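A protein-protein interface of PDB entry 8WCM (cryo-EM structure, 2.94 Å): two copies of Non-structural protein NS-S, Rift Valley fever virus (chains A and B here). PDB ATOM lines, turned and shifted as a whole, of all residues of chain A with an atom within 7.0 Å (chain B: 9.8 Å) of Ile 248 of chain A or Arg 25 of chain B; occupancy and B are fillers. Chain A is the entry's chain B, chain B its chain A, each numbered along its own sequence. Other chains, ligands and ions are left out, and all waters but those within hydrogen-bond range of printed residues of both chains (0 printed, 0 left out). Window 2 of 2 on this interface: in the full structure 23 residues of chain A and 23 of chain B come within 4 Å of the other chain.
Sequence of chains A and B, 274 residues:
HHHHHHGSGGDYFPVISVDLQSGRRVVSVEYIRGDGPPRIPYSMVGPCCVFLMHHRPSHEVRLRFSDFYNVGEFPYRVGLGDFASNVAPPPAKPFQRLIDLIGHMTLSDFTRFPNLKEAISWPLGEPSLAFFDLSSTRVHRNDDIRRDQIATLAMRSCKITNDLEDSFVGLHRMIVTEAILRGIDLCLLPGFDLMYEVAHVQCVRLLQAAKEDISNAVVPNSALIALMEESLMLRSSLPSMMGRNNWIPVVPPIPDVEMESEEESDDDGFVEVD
Among the printed residues, merely in contact across the chains: Arg 182 of chain A with Lys 159 of chain B (3.6 Å), Arg 182 of chain A with Ile 160 of chain B (3.5 Å), Asn 246 of chain A with Ile 160 of chain B (3.7 Å), Asn 246 of chain A with Thr 161 of chain B (3.3 Å), Ile 248 of chain A with Arg 25 of chain B (3.5 Å), Ile 248 of chain A with Val 27 of chain B (3.6 Å), Ile 248 of chain A with Lys 159 of chain B (3.2 Å), Ile 248 of chain A with Thr 161 of chain B (3.4 Å), Pro 249 of chain A with Arg 25 of chain B (3.5 Å), Val 251 of chain A with Gly 23 of chain B (3.3 Å) and Val 251 of chain A with Arg 25 of chain B (3.3 Å).
No position is printed for both chains.
Of the 12 pairs that touch across the chains among the printed residues, none has its exchanged pair printed and touching as well.
Of the printed residues of chain B, Arg 182 of chain A touches Lys 159 and Ile 160.
No residue of chain B comes within 4 Å of Trp 247 of chain A.
Of chain B, only Arg 25, Val 27, Lys 159 and Thr 161 come within 4 Å of Ile 248 of chain A.
Asp 19 of chain B touches none of the printed residues of chain A.
Arg 25 of chain B touches just these residues of chain A: Ile 248, Pro 249 and Val 251.
Printed residues of chain A within 4 Å of Val 27 of chain B: Ile 248.
Ala 154 of chain B touches none of the printed residues of chain A.
Printed residues of chain A within 4 Å of Asn 162 of chain B: Asn 246.
The nearest residue of chain B that does not touch Ile 248 of chain A is Ile 160 of chain B (4.1 Å).
O of Val 27 of chain B lies within hydrogen-bond range of NE of Arg 156 of chain B (2.8 Å).
NZ of Lys 159 of chain B is in hydrogen-bond range of O of Ser 157 of chain B, at 3.3 Å.
NH1 of Arg 182 of chain A is in hydrogen-bond range of O of Asn 246 of chain A (3.0 Å).
The side-chain amide nitrogen (ND2) of Asn 246 of chain A is in hydrogen-bond range of the side-chain amide oxygen (OD1) of Asn 162 of chain B (3.1 Å).
Printed residues of chain A that touch a printed residue of chain B: Arg 182, Asn 246, Ile 248, Pro 249 and Val 251.
Hydrophobic or aromatic side chains of chain A that line the printed part of chain B: Ile 248, Pro 249 and Val 251.
Among the printed residues, 12 pairs touch across the chains.
Among the printed residues, no Asp or Glu carboxylate lies within 4 Å of a Lys or Arg side-chain nitrogen of the other chain.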
ATOM      1  N   ASN A 115     -17.910 -17.468 -16.240  1.00  0.00           N
ATOM      2  CA  ASN A 115     -16.841 -16.646 -16.786  1.00  0.00           C
ATOM      3  C   ASN A 115     -17.299 -15.871 -18.013  1.00  0.00           C
ATOM      4  O   ASN A 115     -16.930 -14.707 -18.182  1.00  0.00           O
ATOM      5  CB  ASN A 115     -15.635 -17.519 -17.109  1.00  0.00           C
ATOM      6  CG  ASN A 115     -14.759 -17.754 -15.906  1.00  0.00           C
ATOM      7  OD1 ASN A 115     -13.986 -16.888 -15.512  1.00  0.00           O
ATOM      8  ND2 ASN A 115     -14.881 -18.924 -15.308  1.00  0.00           N
ATOM      9  N   GLU A 118     -19.360 -12.956 -16.778  1.00  0.00           N
ATOM     10  CA  GLU A 118     -18.495 -11.881 -16.312  1.00  0.00           C
ATOM     11  C   GLU A 118     -17.844 -11.154 -17.478  1.00  0.00           C
ATOM     12  O   GLU A 118     -17.691  -9.929 -17.448  1.00  0.00           O
ATOM     13  CB  GLU A 118     -17.434 -12.437 -15.369  1.00  0.00           C
ATOM     14  CG  GLU A 118     -16.495 -11.391 -14.825  1.00  0.00           C
ATOM     15  CD  GLU A 118     -17.223 -10.281 -14.099  1.00  0.00           C
ATOM     16  OE1 GLU A 118     -18.204 -10.579 -13.387  1.00  0.00           O
ATOM     17  OE2 GLU A 118     -16.814  -9.109 -14.237  1.00  0.00           O
ATOM     18  N   ARG A 182      -6.098  -5.134 -20.713  1.00  0.00           N
ATOM     19  CA  ARG A 182      -6.071  -6.455 -21.321  1.00  0.00           C
ATOM     20  C   ARG A 182      -5.001  -6.600 -22.387  1.00  0.00           C
ATOM     21  O   ARG A 182      -4.937  -7.644 -23.035  1.00  0.00           O
ATOM     22  CB  ARG A 182      -7.430  -6.785 -21.927  1.00  0.00           C
ATOM     23  CG  ARG A 182      -8.578  -6.633 -20.977  1.00  0.00           C
ATOM     24  CD  ARG A 182      -8.719  -7.844 -20.101  1.00  0.00           C
ATOM     25  NE  ARG A 182      -9.683  -7.619 -19.038  1.00  0.00           N
ATOM     26  CZ  ARG A 182      -9.581  -8.138 -17.824  1.00  0.00           C
ATOM     27  NH1 ARG A 182      -8.557  -8.913 -17.524  1.00  0.00           N
ATOM     28  NH2 ARG A 182     -10.503  -7.883 -16.912  1.00  0.00           N
ATOM     29  N   GLU A 212     -10.922 -20.438 -18.877  1.00  0.00           N
ATOM     30  CA  GLU A 212     -11.326 -20.876 -17.548  1.00  0.00           C
ATOM     31  C   GLU A 212     -12.607 -21.690 -17.596  1.00  0.00           C
ATOM     32  O   GLU A 212     -12.783 -22.614 -16.797  1.00  0.00           O
ATOM     33  CB  GLU A 212     -11.499 -19.677 -16.621  1.00  0.00           C
ATOM     34  CG  GLU A 212     -10.375 -18.669 -16.710  1.00  0.00           C
ATOM     35  CD  GLU A 212      -9.120 -19.135 -16.004  1.00  0.00           C
ATOM     36  OE1 GLU A 212      -8.062 -18.499 -16.195  1.00  0.00           O
ATOM     37  OE2 GLU A 212      -9.190 -20.131 -15.256  1.00  0.00           O
ATOM     38  N   ASN A 216     -12.986 -25.484 -16.282  1.00  0.00           N
ATOM     39  CA  ASN A 216     -13.971 -25.906 -15.297  1.00  0.00           C
ATOM     40  C   ASN A 216     -14.810 -27.081 -15.774  1.00  0.00           C
ATOM     41  O   ASN A 216     -15.728 -27.495 -15.059  1.00  0.00           O
ATOM     42  CB  ASN A 216     -14.889 -24.739 -14.928  1.00  0.00           C
ATOM     43  CG  ASN A 216     -14.262 -23.811 -13.913  1.00  0.00           C
ATOM     44  OD1 ASN A 216     -13.202 -24.103 -13.362  1.00  0.00           O
ATOM     45  ND2 ASN A 216     -14.916 -22.685 -13.657  1.00  0.00           N
ATOM     46  N   ASN A 246      -4.481 -12.383 -18.154  1.00  0.00           N
ATOM     47  CA  ASN A 246      -4.671 -11.794 -16.834  1.00  0.00           C
ATOM     48  C   ASN A 246      -6.146 -11.743 -16.483  1.00  0.00           C
ATOM     49  O   ASN A 246      -6.671 -10.722 -16.046  1.00  0.00           O
ATOM     50  CB  ASN A 246      -4.050 -10.406 -16.753  1.00  0.00           C
ATOM     51  CG  ASN A 246      -4.501  -9.496 -17.866  1.00  0.00           C
ATOM     52  OD1 ASN A 246      -5.489  -9.762 -18.537  1.00  0.00           O
ATOM     53  ND2 ASN A 246      -3.775  -8.409 -18.066  1.00  0.00           N
ATOM     54  N   TRP A 247      -6.841 -12.853 -16.675  1.00  0.00           N
ATOM     55  CA  TRP A 247      -8.254 -12.946 -16.349  1.00  0.00           C
ATOM     56  C   TRP A 247      -8.413 -13.592 -14.981  1.00  0.00           C
ATOM     57  O   TRP A 247      -7.870 -14.673 -14.737  1.00  0.00           O
ATOM     58  CB  TRP A 247      -8.998 -13.754 -17.410  1.00  0.00           C
ATOM     59  CG  TRP A 247     -10.422 -13.988 -17.083  1.00  0.00           C
ATOM     60  CD1 TRP A 247     -10.956 -15.088 -16.494  1.00  0.00           C
ATOM     61  CD2 TRP A 247     -11.508 -13.097 -17.326  1.00  0.00           C
ATOM     62  NE1 TRP A 247     -12.308 -14.940 -16.352  1.00  0.00           N
ATOM     63  CE2 TRP A 247     -12.672 -13.721 -16.855  1.00  0.00           C
ATOM     64  CE3 TRP A 247     -11.609 -11.829 -17.895  1.00  0.00           C
ATOM     65  CZ2 TRP A 247     -13.916 -13.122 -16.934  1.00  0.00           C
ATOM     66  CZ3 TRP A 247     -12.840 -11.239 -17.971  1.00  0.00           C
ATOM     67  CH2 TRP A 247     -13.979 -11.882 -17.496  1.00  0.00           C
ATOM     68  N   ILE A 248      -9.146 -12.931 -14.089  1.00  0.00           N
ATOM     69  CA  ILE A 248      -9.437 -13.492 -12.773  1.00  0.00           C
ATOM     70  C   ILE A 248     -10.523 -14.546 -12.929  1.00  0.00           C
ATOM     71  O   ILE A 248     -11.632 -14.219 -13.369  1.00  0.00           O
ATOM     72  CB  ILE A 248      -9.898 -12.422 -11.774  1.00  0.00           C
ATOM     73  CG1 ILE A 248      -8.927 -11.255 -11.720  1.00  0.00           C
ATOM     74  CG2 ILE A 248     -10.028 -13.021 -10.396  1.00  0.00           C
ATOM     75  CD1 ILE A 248      -9.445 -10.106 -10.919  1.00  0.00           C
ATOM     76  N   PRO A 249     -10.265 -15.801 -12.581  1.00  0.00           N
ATOM     77  CA  PRO A 249     -11.322 -16.811 -12.669  1.00  0.00           C
ATOM     78  C   PRO A 249     -12.466 -16.485 -11.725  1.00  0.00           C
ATOM     79  O   PRO A 249     -12.260 -15.994 -10.616  1.00  0.00           O
ATOM     80  CB  PRO A 249     -10.611 -18.104 -12.265  1.00  0.00           C
ATOM     81  CG  PRO A 249      -9.163 -17.817 -12.431  1.00  0.00           C
ATOM     82  CD  PRO A 249      -8.991 -16.375 -12.130  1.00  0.00           C
ATOM     83  N   VAL A 250     -13.678 -16.763 -12.177  1.00  0.00           N
ATOM     84  CA  VAL A 250     -14.879 -16.494 -11.399  1.00  0.00           C
ATOM     85  C   VAL A 250     -15.259 -17.758 -10.645  1.00  0.00           C
ATOM     86  O   VAL A 250     -15.323 -18.844 -11.232  1.00  0.00           O
ATOM     87  CB  VAL A 250     -16.026 -16.026 -12.308  1.00  0.00           C
ATOM     88  CG1 VAL A 250     -17.359 -16.207 -11.618  1.00  0.00           C
ATOM     89  CG2 VAL A 250     -15.823 -14.582 -12.705  1.00  0.00           C
ATOM     90  N   VAL A 251     -15.494 -17.626  -9.346  1.00  0.00           N
ATOM     91  CA  VAL A 251     -15.890 -18.787  -8.542  1.00  0.00           C
ATOM     92  C   VAL A 251     -17.263 -19.270  -8.994  1.00  0.00           C
ATOM     93  O   VAL A 251     -18.200 -18.459  -9.110  1.00  0.00           O
ATOM     94  CB  VAL A 251     -15.879 -18.434  -7.052  1.00  0.00           C
ATOM     95  CG1 VAL A 251     -14.467 -18.134  -6.601  1.00  0.00           C
ATOM     96  CG2 VAL A 251     -16.760 -17.229  -6.775  1.00  0.00           C
ATOM     97  N   PRO A 252     -17.429 -20.554  -9.292  1.00  0.00           N
ATOM     98  CA  PRO A 252     -18.720 -21.046  -9.770  1.00  0.00           C
ATOM     99  C   PRO A 252     -19.742 -21.066  -8.649  1.00  0.00           C
ATOM    100  O   PRO A 252     -19.489 -21.634  -7.577  1.00  0.00           O
ATOM    101  CB  PRO A 252     -18.402 -22.467 -10.260  1.00  0.00           C
ATOM    102  CG  PRO A 252     -16.908 -22.526 -10.370  1.00  0.00           C
ATOM    103  CD  PRO A 252     -16.396 -21.599  -9.323  1.00  0.00           C
ATOM    104  N   ILE B  16       2.137 -10.571  -6.618  1.00  0.00           N
ATOM    105  CA  ILE B  16       0.702 -10.532  -6.838  1.00  0.00           C
ATOM    106  C   ILE B  16       0.164 -11.946  -6.717  1.00  0.00           C
ATOM    107  O   ILE B  16       0.629 -12.857  -7.410  1.00  0.00           O
ATOM    108  CB  ILE B  16       0.372  -9.927  -8.211  1.00  0.00           C
ATOM    109  CG1 ILE B  16       1.017  -8.551  -8.340  1.00  0.00           C
ATOM    110  CG2 ILE B  16      -1.112  -9.829  -8.394  1.00  0.00           C
ATOM    111  CD1 ILE B  16       1.321  -8.153  -9.747  1.00  0.00           C
ATOM    112  N   SER B  17      -0.810 -12.132  -5.835  1.00  0.00           N
ATOM    113  CA  SER B  17      -1.345 -13.450  -5.543  1.00  0.00           C
ATOM    114  C   SER B  17      -2.860 -13.406  -5.613  1.00  0.00           C
ATOM    115  O   SER B  17      -3.486 -12.526  -5.019  1.00  0.00           O
ATOM    116  CB  SER B  17      -0.890 -13.930  -4.164  1.00  0.00           C
ATOM    117  OG  SER B  17      -1.058 -12.914  -3.193  1.00  0.00           O
ATOM    118  N   VAL B  18      -3.442 -14.354  -6.331  1.00  0.00           N
ATOM    119  CA  VAL B  18      -4.888 -14.442  -6.475  1.00  0.00           C
ATOM    120  C   VAL B  18      -5.380 -15.545  -5.551  1.00  0.00           C
ATOM    121  O   VAL B  18      -5.048 -16.719  -5.744  1.00  0.00           O
ATOM    122  CB  VAL B  18      -5.279 -14.724  -7.931  1.00  0.00           C
ATOM    123  CG1 VAL B  18      -6.755 -14.981  -8.036  1.00  0.00           C
ATOM    124  CG2 VAL B  18      -4.870 -13.571  -8.815  1.00  0.00           C
ATOM    125  N   ASP B  19      -6.171 -15.176  -4.548  1.00  0.00           N
ATOM    126  CA  ASP B  19      -6.550 -16.100  -3.491  1.00  0.00           C
ATOM    127  C   ASP B  19      -8.047 -16.015  -3.239  1.00  0.00           C
ATOM    128  O   ASP B  19      -8.692 -15.012  -3.544  1.00  0.00           O
ATOM    129  CB  ASP B  19      -5.791 -15.805  -2.191  1.00  0.00           C
ATOM    130  CG  ASP B  19      -4.284 -15.850  -2.369  1.00  0.00           C
ATOM    131  OD1 ASP B  19      -3.579 -15.119  -1.643  1.00  0.00           O
ATOM    132  OD2 ASP B  19      -3.802 -16.616  -3.227  1.00  0.00           O
ATOM    133  N   LEU B  20      -8.597 -17.081  -2.668  1.00  0.00           N
ATOM    134  CA  LEU B  20     -10.021 -17.147  -2.366  1.00  0.00           C
ATOM    135  C   LEU B  20     -10.280 -16.553  -0.985  1.00  0.00           C
ATOM    136  O   LEU B  20      -9.685 -16.989   0.004  1.00  0.00           O
ATOM    137  CB  LEU B  20     -10.524 -18.589  -2.427  1.00  0.00           C
ATOM    138  CG  LEU B  20     -10.855 -19.150  -3.809  1.00  0.00           C
ATOM    139  CD1 LEU B  20      -9.589 -19.501  -4.574  1.00  0.00           C
ATOM    140  CD2 LEU B  20     -11.764 -20.358  -3.688  1.00  0.00           C
ATOM    141  N   GLN B  21     -11.168 -15.563  -0.922  1.00  0.00           N
ATOM    142  CA  GLN B  21     -11.579 -14.946   0.331  1.00  0.00           C
ATOM    143  C   GLN B  21     -13.063 -14.628   0.247  1.00  0.00           C
ATOM    144  O   GLN B  21     -13.517 -14.046  -0.742  1.00  0.00           O
ATOM    145  CB  GLN B  21     -10.782 -13.668   0.616  1.00  0.00           C
ATOM    146  CG  GLN B  21      -9.313 -13.899   0.928  1.00  0.00           C
ATOM    147  CD  GLN B  21      -8.517 -12.610   0.977  1.00  0.00           C
ATOM    148  OE1 GLN B  21      -9.074 -11.529   1.167  1.00  0.00           O
ATOM    149  NE2 GLN B  21      -7.206 -12.719   0.800  1.00  0.00           N
ATOM    150  N   SER B  22     -13.811 -15.017   1.280  1.00  0.00           N
ATOM    151  CA  SER B  22     -15.238 -14.708   1.385  1.00  0.00           C
ATOM    152  C   SER B  22     -16.016 -15.223   0.176  1.00  0.00           C
ATOM    153  O   SER B  22     -16.960 -14.587  -0.296  1.00  0.00           O
ATOM    154  CB  SER B  22     -15.463 -13.206   1.572  1.00  0.00           C
ATOM    155  OG  SER B  22     -16.842 -12.886   1.525  1.00  0.00           O
ATOM    156  N   GLY B  23     -15.620 -16.388  -0.327  1.00  0.00           N
ATOM    157  CA  GLY B  23     -16.289 -16.955  -1.488  1.00  0.00           C
ATOM    158  C   GLY B  23     -16.098 -16.151  -2.754  1.00  0.00           C
ATOM    159  O   GLY B  23     -16.946 -16.205  -3.654  1.00  0.00           O
ATOM    160  N   ARG B  24     -15.005 -15.398  -2.842  1.00  0.00           N
ATOM    161  CA  ARG B  24     -14.682 -14.635  -4.040  1.00  0.00           C
ATOM    162  C   ARG B  24     -13.187 -14.737  -4.284  1.00  0.00           C
ATOM    163  O   ARG B  24     -12.398 -14.612  -3.346  1.00  0.00           O
ATOM    164  CB  ARG B  24     -15.096 -13.167  -3.899  1.00  0.00           C
ATOM    165  CG  ARG B  24     -16.573 -12.917  -4.130  1.00  0.00           C
ATOM    166  CD  ARG B  24     -16.934 -13.084  -5.597  1.00  0.00           C
ATOM    167  NE  ARG B  24     -18.365 -12.908  -5.833  1.00  0.00           N
ATOM    168  CZ  ARG B  24     -18.973 -11.729  -5.918  1.00  0.00           C
ATOM    169  NH1 ARG B  24     -18.277 -10.609  -5.790  1.00  0.00           N
ATOM    170  NH2 ARG B  24     -20.280 -11.669  -6.134  1.00  0.00           N
ATOM    171  N   ARG B  25     -12.801 -14.967  -5.533  1.00  0.00           N
ATOM    172  CA  ARG B  25     -11.389 -15.036  -5.871  1.00  0.00           C
ATOM    173  C   ARG B  25     -10.883 -13.628  -6.154  1.00  0.00           C
ATOM    174  O   ARG B  25     -11.321 -12.988  -7.115  1.00  0.00           O
ATOM    175  CB  ARG B  25     -11.174 -15.963  -7.063  1.00  0.00           C
ATOM    176  CG  ARG B  25      -9.759 -16.464  -7.177  1.00  0.00           C
ATOM    177  CD  ARG B  25      -9.552 -17.285  -8.426  1.00  0.00           C
ATOM    178  NE  ARG B  25      -9.646 -18.713  -8.147  1.00  0.00           N
ATOM    179  CZ  ARG B  25     -10.770 -19.417  -8.212  1.00  0.00           C
ATOM    180  NH1 ARG B  25     -11.906 -18.828  -8.549  1.00  0.00           N
ATOM    181  NH2 ARG B  25     -10.754 -20.712  -7.939  1.00  0.00           N
ATOM    182  N   VAL B  26      -9.970 -13.146  -5.315  1.00  0.00           N
ATOM    183  CA  VAL B  26      -9.590 -11.742  -5.285  1.00  0.00           C
ATOM    184  C   VAL B  26      -8.075 -11.627  -5.362  1.00  0.00           C
ATOM    185  O   VAL B  26      -7.338 -12.511  -4.912  1.00  0.00           O
ATOM    186  CB  VAL B  26     -10.134 -11.056  -4.013  1.00  0.00           C
ATOM    187  CG1 VAL B  26      -9.484 -11.645  -2.772  1.00  0.00           C
ATOM    188  CG2 VAL B  26      -9.959  -9.550  -4.080  1.00  0.00           C
ATOM    189  N   VAL B  27      -7.615 -10.526  -5.938  1.00  0.00           N
ATOM    190  CA  VAL B  27      -6.200 -10.250  -6.138  1.00  0.00           C
ATOM    191  C   VAL B  27      -5.656  -9.504  -4.933  1.00  0.00           C
ATOM    192  O   VAL B  27      -6.335  -8.650  -4.356  1.00  0.00           O
ATOM    193  CB  VAL B  27      -5.989  -9.438  -7.426  1.00  0.00           C
ATOM    194  CG1 VAL B  27      -4.525  -9.316  -7.742  1.00  0.00           C
ATOM    195  CG2 VAL B  27      -6.718 -10.088  -8.568  1.00  0.00           C
ATOM    196  N   SER B  28      -4.424  -9.820  -4.549  1.00  0.00           N
ATOM    197  CA  SER B  28      -3.733  -9.094  -3.500  1.00  0.00           C
ATOM    198  C   SER B  28      -2.293  -8.884  -3.928  1.00  0.00           C
ATOM    199  O   SER B  28      -1.759  -9.636  -4.741  1.00  0.00           O
ATOM    200  CB  SER B  28      -3.787  -9.845  -2.169  1.00  0.00           C
ATOM    201  OG  SER B  28      -5.110  -9.883  -1.668  1.00  0.00           O
ATOM    202  N   LEU B 124     -14.431  -0.159  -7.280  1.00  0.00           N
ATOM    203  CA  LEU B 124     -14.227  -1.593  -7.130  1.00  0.00           C
ATOM    204  C   LEU B 124     -15.447  -2.413  -7.518  1.00  0.00           C
ATOM    205  O   LEU B 124     -15.354  -3.641  -7.563  1.00  0.00           O
ATOM    206  CB  LEU B 124     -13.834  -1.920  -5.691  1.00  0.00           C
ATOM    207  CG  LEU B 124     -12.671  -1.147  -5.075  1.00  0.00           C
ATOM    208  CD1 LEU B 124     -12.406  -1.648  -3.683  1.00  0.00           C
ATOM    209  CD2 LEU B 124     -11.433  -1.275  -5.912  1.00  0.00           C
ATOM    210  N   GLU B 126     -18.013  -2.787  -5.688  1.00  0.00           N
ATOM    211  CA  GLU B 126     -18.622  -3.162  -4.426  1.00  0.00           C
ATOM    212  C   GLU B 126     -18.415  -2.020  -3.445  1.00  0.00           C
ATOM    213  O   GLU B 126     -17.444  -1.266  -3.573  1.00  0.00           O
ATOM    214  CB  GLU B 126     -17.995  -4.442  -3.863  1.00  0.00           C
ATOM    215  CG  GLU B 126     -16.495  -4.332  -3.704  1.00  0.00           C
ATOM    216  CD  GLU B 126     -15.876  -5.583  -3.133  1.00  0.00           C
ATOM    217  OE1 GLU B 126     -16.632  -6.500  -2.752  1.00  0.00           O
ATOM    218  OE2 GLU B 126     -14.632  -5.654  -3.073  1.00  0.00           O
ATOM    219  N   THR B 152      -2.781  -3.168  -3.676  1.00  0.00           N
ATOM    220  CA  THR B 152      -3.913  -4.081  -3.744  1.00  0.00           C
ATOM    221  C   THR B 152      -5.155  -3.386  -4.279  1.00  0.00           C
ATOM    222  O   THR B 152      -5.892  -3.958  -5.084  1.00  0.00           O
ATOM    223  CB  THR B 152      -4.190  -4.665  -2.365  1.00  0.00           C
ATOM    224  OG1 THR B 152      -3.029  -5.358  -1.902  1.00  0.00           O
ATOM    225  CG2 THR B 152      -5.343  -5.622  -2.424  1.00  0.00           C
ATOM    226  N   ALA B 154      -5.245  -0.651  -6.189  1.00  0.00           N
ATOM    227  CA  ALA B 154      -5.029  -0.373  -7.602  1.00  0.00           C
ATOM    228  C   ALA B 154      -5.294  -1.609  -8.447  1.00  0.00           C
ATOM    229  O   ALA B 154      -5.897  -1.516  -9.518  1.00  0.00           O
ATOM    230  CB  ALA B 154      -3.611   0.135  -7.834  1.00  0.00           C
ATOM    231  N   MET B 155      -4.852  -2.778  -7.982  1.00  0.00           N
ATOM    232  CA  MET B 155      -5.080  -4.005  -8.739  1.00  0.00           C
ATOM    233  C   MET B 155      -6.552  -4.398  -8.742  1.00  0.00           C
ATOM    234  O   MET B 155      -7.070  -4.847  -9.766  1.00  0.00           O
ATOM    235  CB  MET B 155      -4.237  -5.139  -8.167  1.00  0.00           C
ATOM    236  CG  MET B 155      -2.764  -5.050  -8.502  1.00  0.00           C
ATOM    237  SD  MET B 155      -2.382  -5.314 -10.233  1.00  0.00           S
ATOM    238  CE  MET B 155      -2.751  -7.046 -10.383  1.00  0.00           C
ATOM    239  N   ARG B 156      -7.236  -4.251  -7.610  1.00  0.00           N
ATOM    240  CA  ARG B 156      -8.633  -4.650  -7.502  1.00  0.00           C
ATOM    241  C   ARG B 156      -9.575  -3.719  -8.243  1.00  0.00           C
ATOM    242  O   ARG B 156     -10.676  -4.141  -8.603  1.00  0.00           O
ATOM    243  CB  ARG B 156      -9.049  -4.720  -6.037  1.00  0.00           C
ATOM    244  CG  ARG B 156      -8.523  -5.929  -5.325  1.00  0.00           C
ATOM    245  CD  ARG B 156      -8.882  -5.915  -3.860  1.00  0.00           C
ATOM    246  NE  ARG B 156      -8.196  -6.990  -3.154  1.00  0.00           N
ATOM    247  CZ  ARG B 156      -8.381  -7.286  -1.876  1.00  0.00           C
ATOM    248  NH1 ARG B 156      -9.237  -6.587  -1.149  1.00  0.00           N
ATOM    249  NH2 ARG B 156      -7.708  -8.285  -1.325  1.00  0.00           N
ATOM    250  N   SER B 157      -9.187  -2.464  -8.450  1.00  0.00           N
ATOM    251  CA  SER B 157      -9.980  -1.574  -9.287  1.00  0.00           C
ATOM    252  C   SER B 157     -10.028  -2.054 -10.726  1.00  0.00           C
ATOM    253  O   SER B 157     -11.080  -1.995 -11.367  1.00  0.00           O
ATOM    254  CB  SER B 157      -9.405  -0.165  -9.239  1.00  0.00           C
ATOM    255  OG  SER B 157      -9.394   0.325  -7.917  1.00  0.00           O
ATOM    256  N   CYS B 158      -8.898  -2.534 -11.240  1.00  0.00           N
ATOM    257  CA  CYS B 158      -8.758  -2.910 -12.636  1.00  0.00           C
ATOM    258  C   CYS B 158      -9.146  -4.355 -12.911  1.00  0.00           C
ATOM    259  O   CYS B 158      -9.407  -4.697 -14.066  1.00  0.00           O
ATOM    260  CB  CYS B 158      -7.321  -2.667 -13.082  1.00  0.00           C
ATOM    261  SG  CYS B 158      -6.791  -0.971 -12.852  1.00  0.00           S
ATOM    262  N   LYS B 159      -9.182  -5.204 -11.886  1.00  0.00           N
ATOM    263  CA  LYS B 159      -9.658  -6.581 -11.995  1.00  0.00           C
ATOM    264  C   LYS B 159      -8.776  -7.427 -12.907  1.00  0.00           C
ATOM    265  O   LYS B 159      -9.259  -8.324 -13.598  1.00  0.00           O
ATOM    266  CB  LYS B 159     -11.112  -6.623 -12.464  1.00  0.00           C
ATOM    267  CG  LYS B 159     -12.044  -5.832 -11.583  1.00  0.00           C
ATOM    268  CD  LYS B 159     -13.452  -5.837 -12.121  1.00  0.00           C
ATOM    269  CE  LYS B 159     -14.350  -4.945 -11.292  1.00  0.00           C
ATOM    270  NZ  LYS B 159     -13.983  -3.511 -11.438  1.00  0.00           N
ATOM    271  N   ILE B 160      -7.478  -7.154 -12.910  1.00  0.00           N
ATOM    272  CA  ILE B 160      -6.513  -7.979 -13.622  1.00  0.00           C
ATOM    273  C   ILE B 160      -5.616  -8.656 -12.598  1.00  0.00           C
ATOM    274  O   ILE B 160      -5.721  -8.394 -11.398  1.00  0.00           O
ATOM    275  CB  ILE B 160      -5.704  -7.137 -14.622  1.00  0.00           C
ATOM    276  CG1 ILE B 160      -5.002  -5.996 -13.903  1.00  0.00           C
ATOM    277  CG2 ILE B 160      -6.606  -6.588 -15.692  1.00  0.00           C
ATOM    278  CD1 ILE B 160      -4.064  -5.235 -14.781  1.00  0.00           C
ATOM    279  N   THR B 161      -4.730  -9.540 -13.056  1.00  0.00           N
ATOM    280  CA  THR B 161      -3.923 -10.336 -12.142  1.00  0.00           C
ATOM    281  C   THR B 161      -2.422 -10.193 -12.303  1.00  0.00           C
ATOM    282  O   THR B 161      -1.692 -10.768 -11.491  1.00  0.00           O
ATOM    283  CB  THR B 161      -4.249 -11.827 -12.280  1.00  0.00           C
ATOM    284  OG1 THR B 161      -3.947 -12.260 -13.608  1.00  0.00           O
ATOM    285  CG2 THR B 161      -5.689 -12.085 -12.005  1.00  0.00           C
ATOM    286  N   ASN B 162      -1.926  -9.489 -13.302  1.00  0.00           N
ATOM    287  CA  ASN B 162      -0.507  -9.686 -13.569  1.00  0.00           C
ATOM    288  C   ASN B 162       0.327  -8.416 -13.553  1.00  0.00           C
ATOM    289  O   ASN B 162       1.459  -8.449 -13.066  1.00  0.00           O
ATOM    290  CB  ASN B 162      -0.324 -10.401 -14.917  1.00  0.00           C
ATOM    291  CG  ASN B 162      -0.723  -9.539 -16.092  1.00  0.00           C
ATOM    292  OD1 ASN B 162      -1.493  -8.591 -15.946  1.00  0.00           O
ATOM    293  ND2 ASN B 162      -0.199  -9.863 -17.270  1.00  0.00           N
ATOM    294  N   SER B 167      -1.984  -1.283 -13.750  1.00  0.00           N
ATOM    295  CA  SER B 167      -3.050  -1.079 -12.778  1.00  0.00           C
ATOM    296  C   SER B 167      -3.110   0.368 -12.315  1.00  0.00           C
ATOM    297  O   SER B 167      -4.197   0.926 -12.160  1.00  0.00           O
ATOM    298  CB  SER B 167      -2.862  -2.011 -11.593  1.00  0.00           C
ATOM    299  OG  SER B 167      -3.181  -3.337 -11.958  1.00  0.00           O
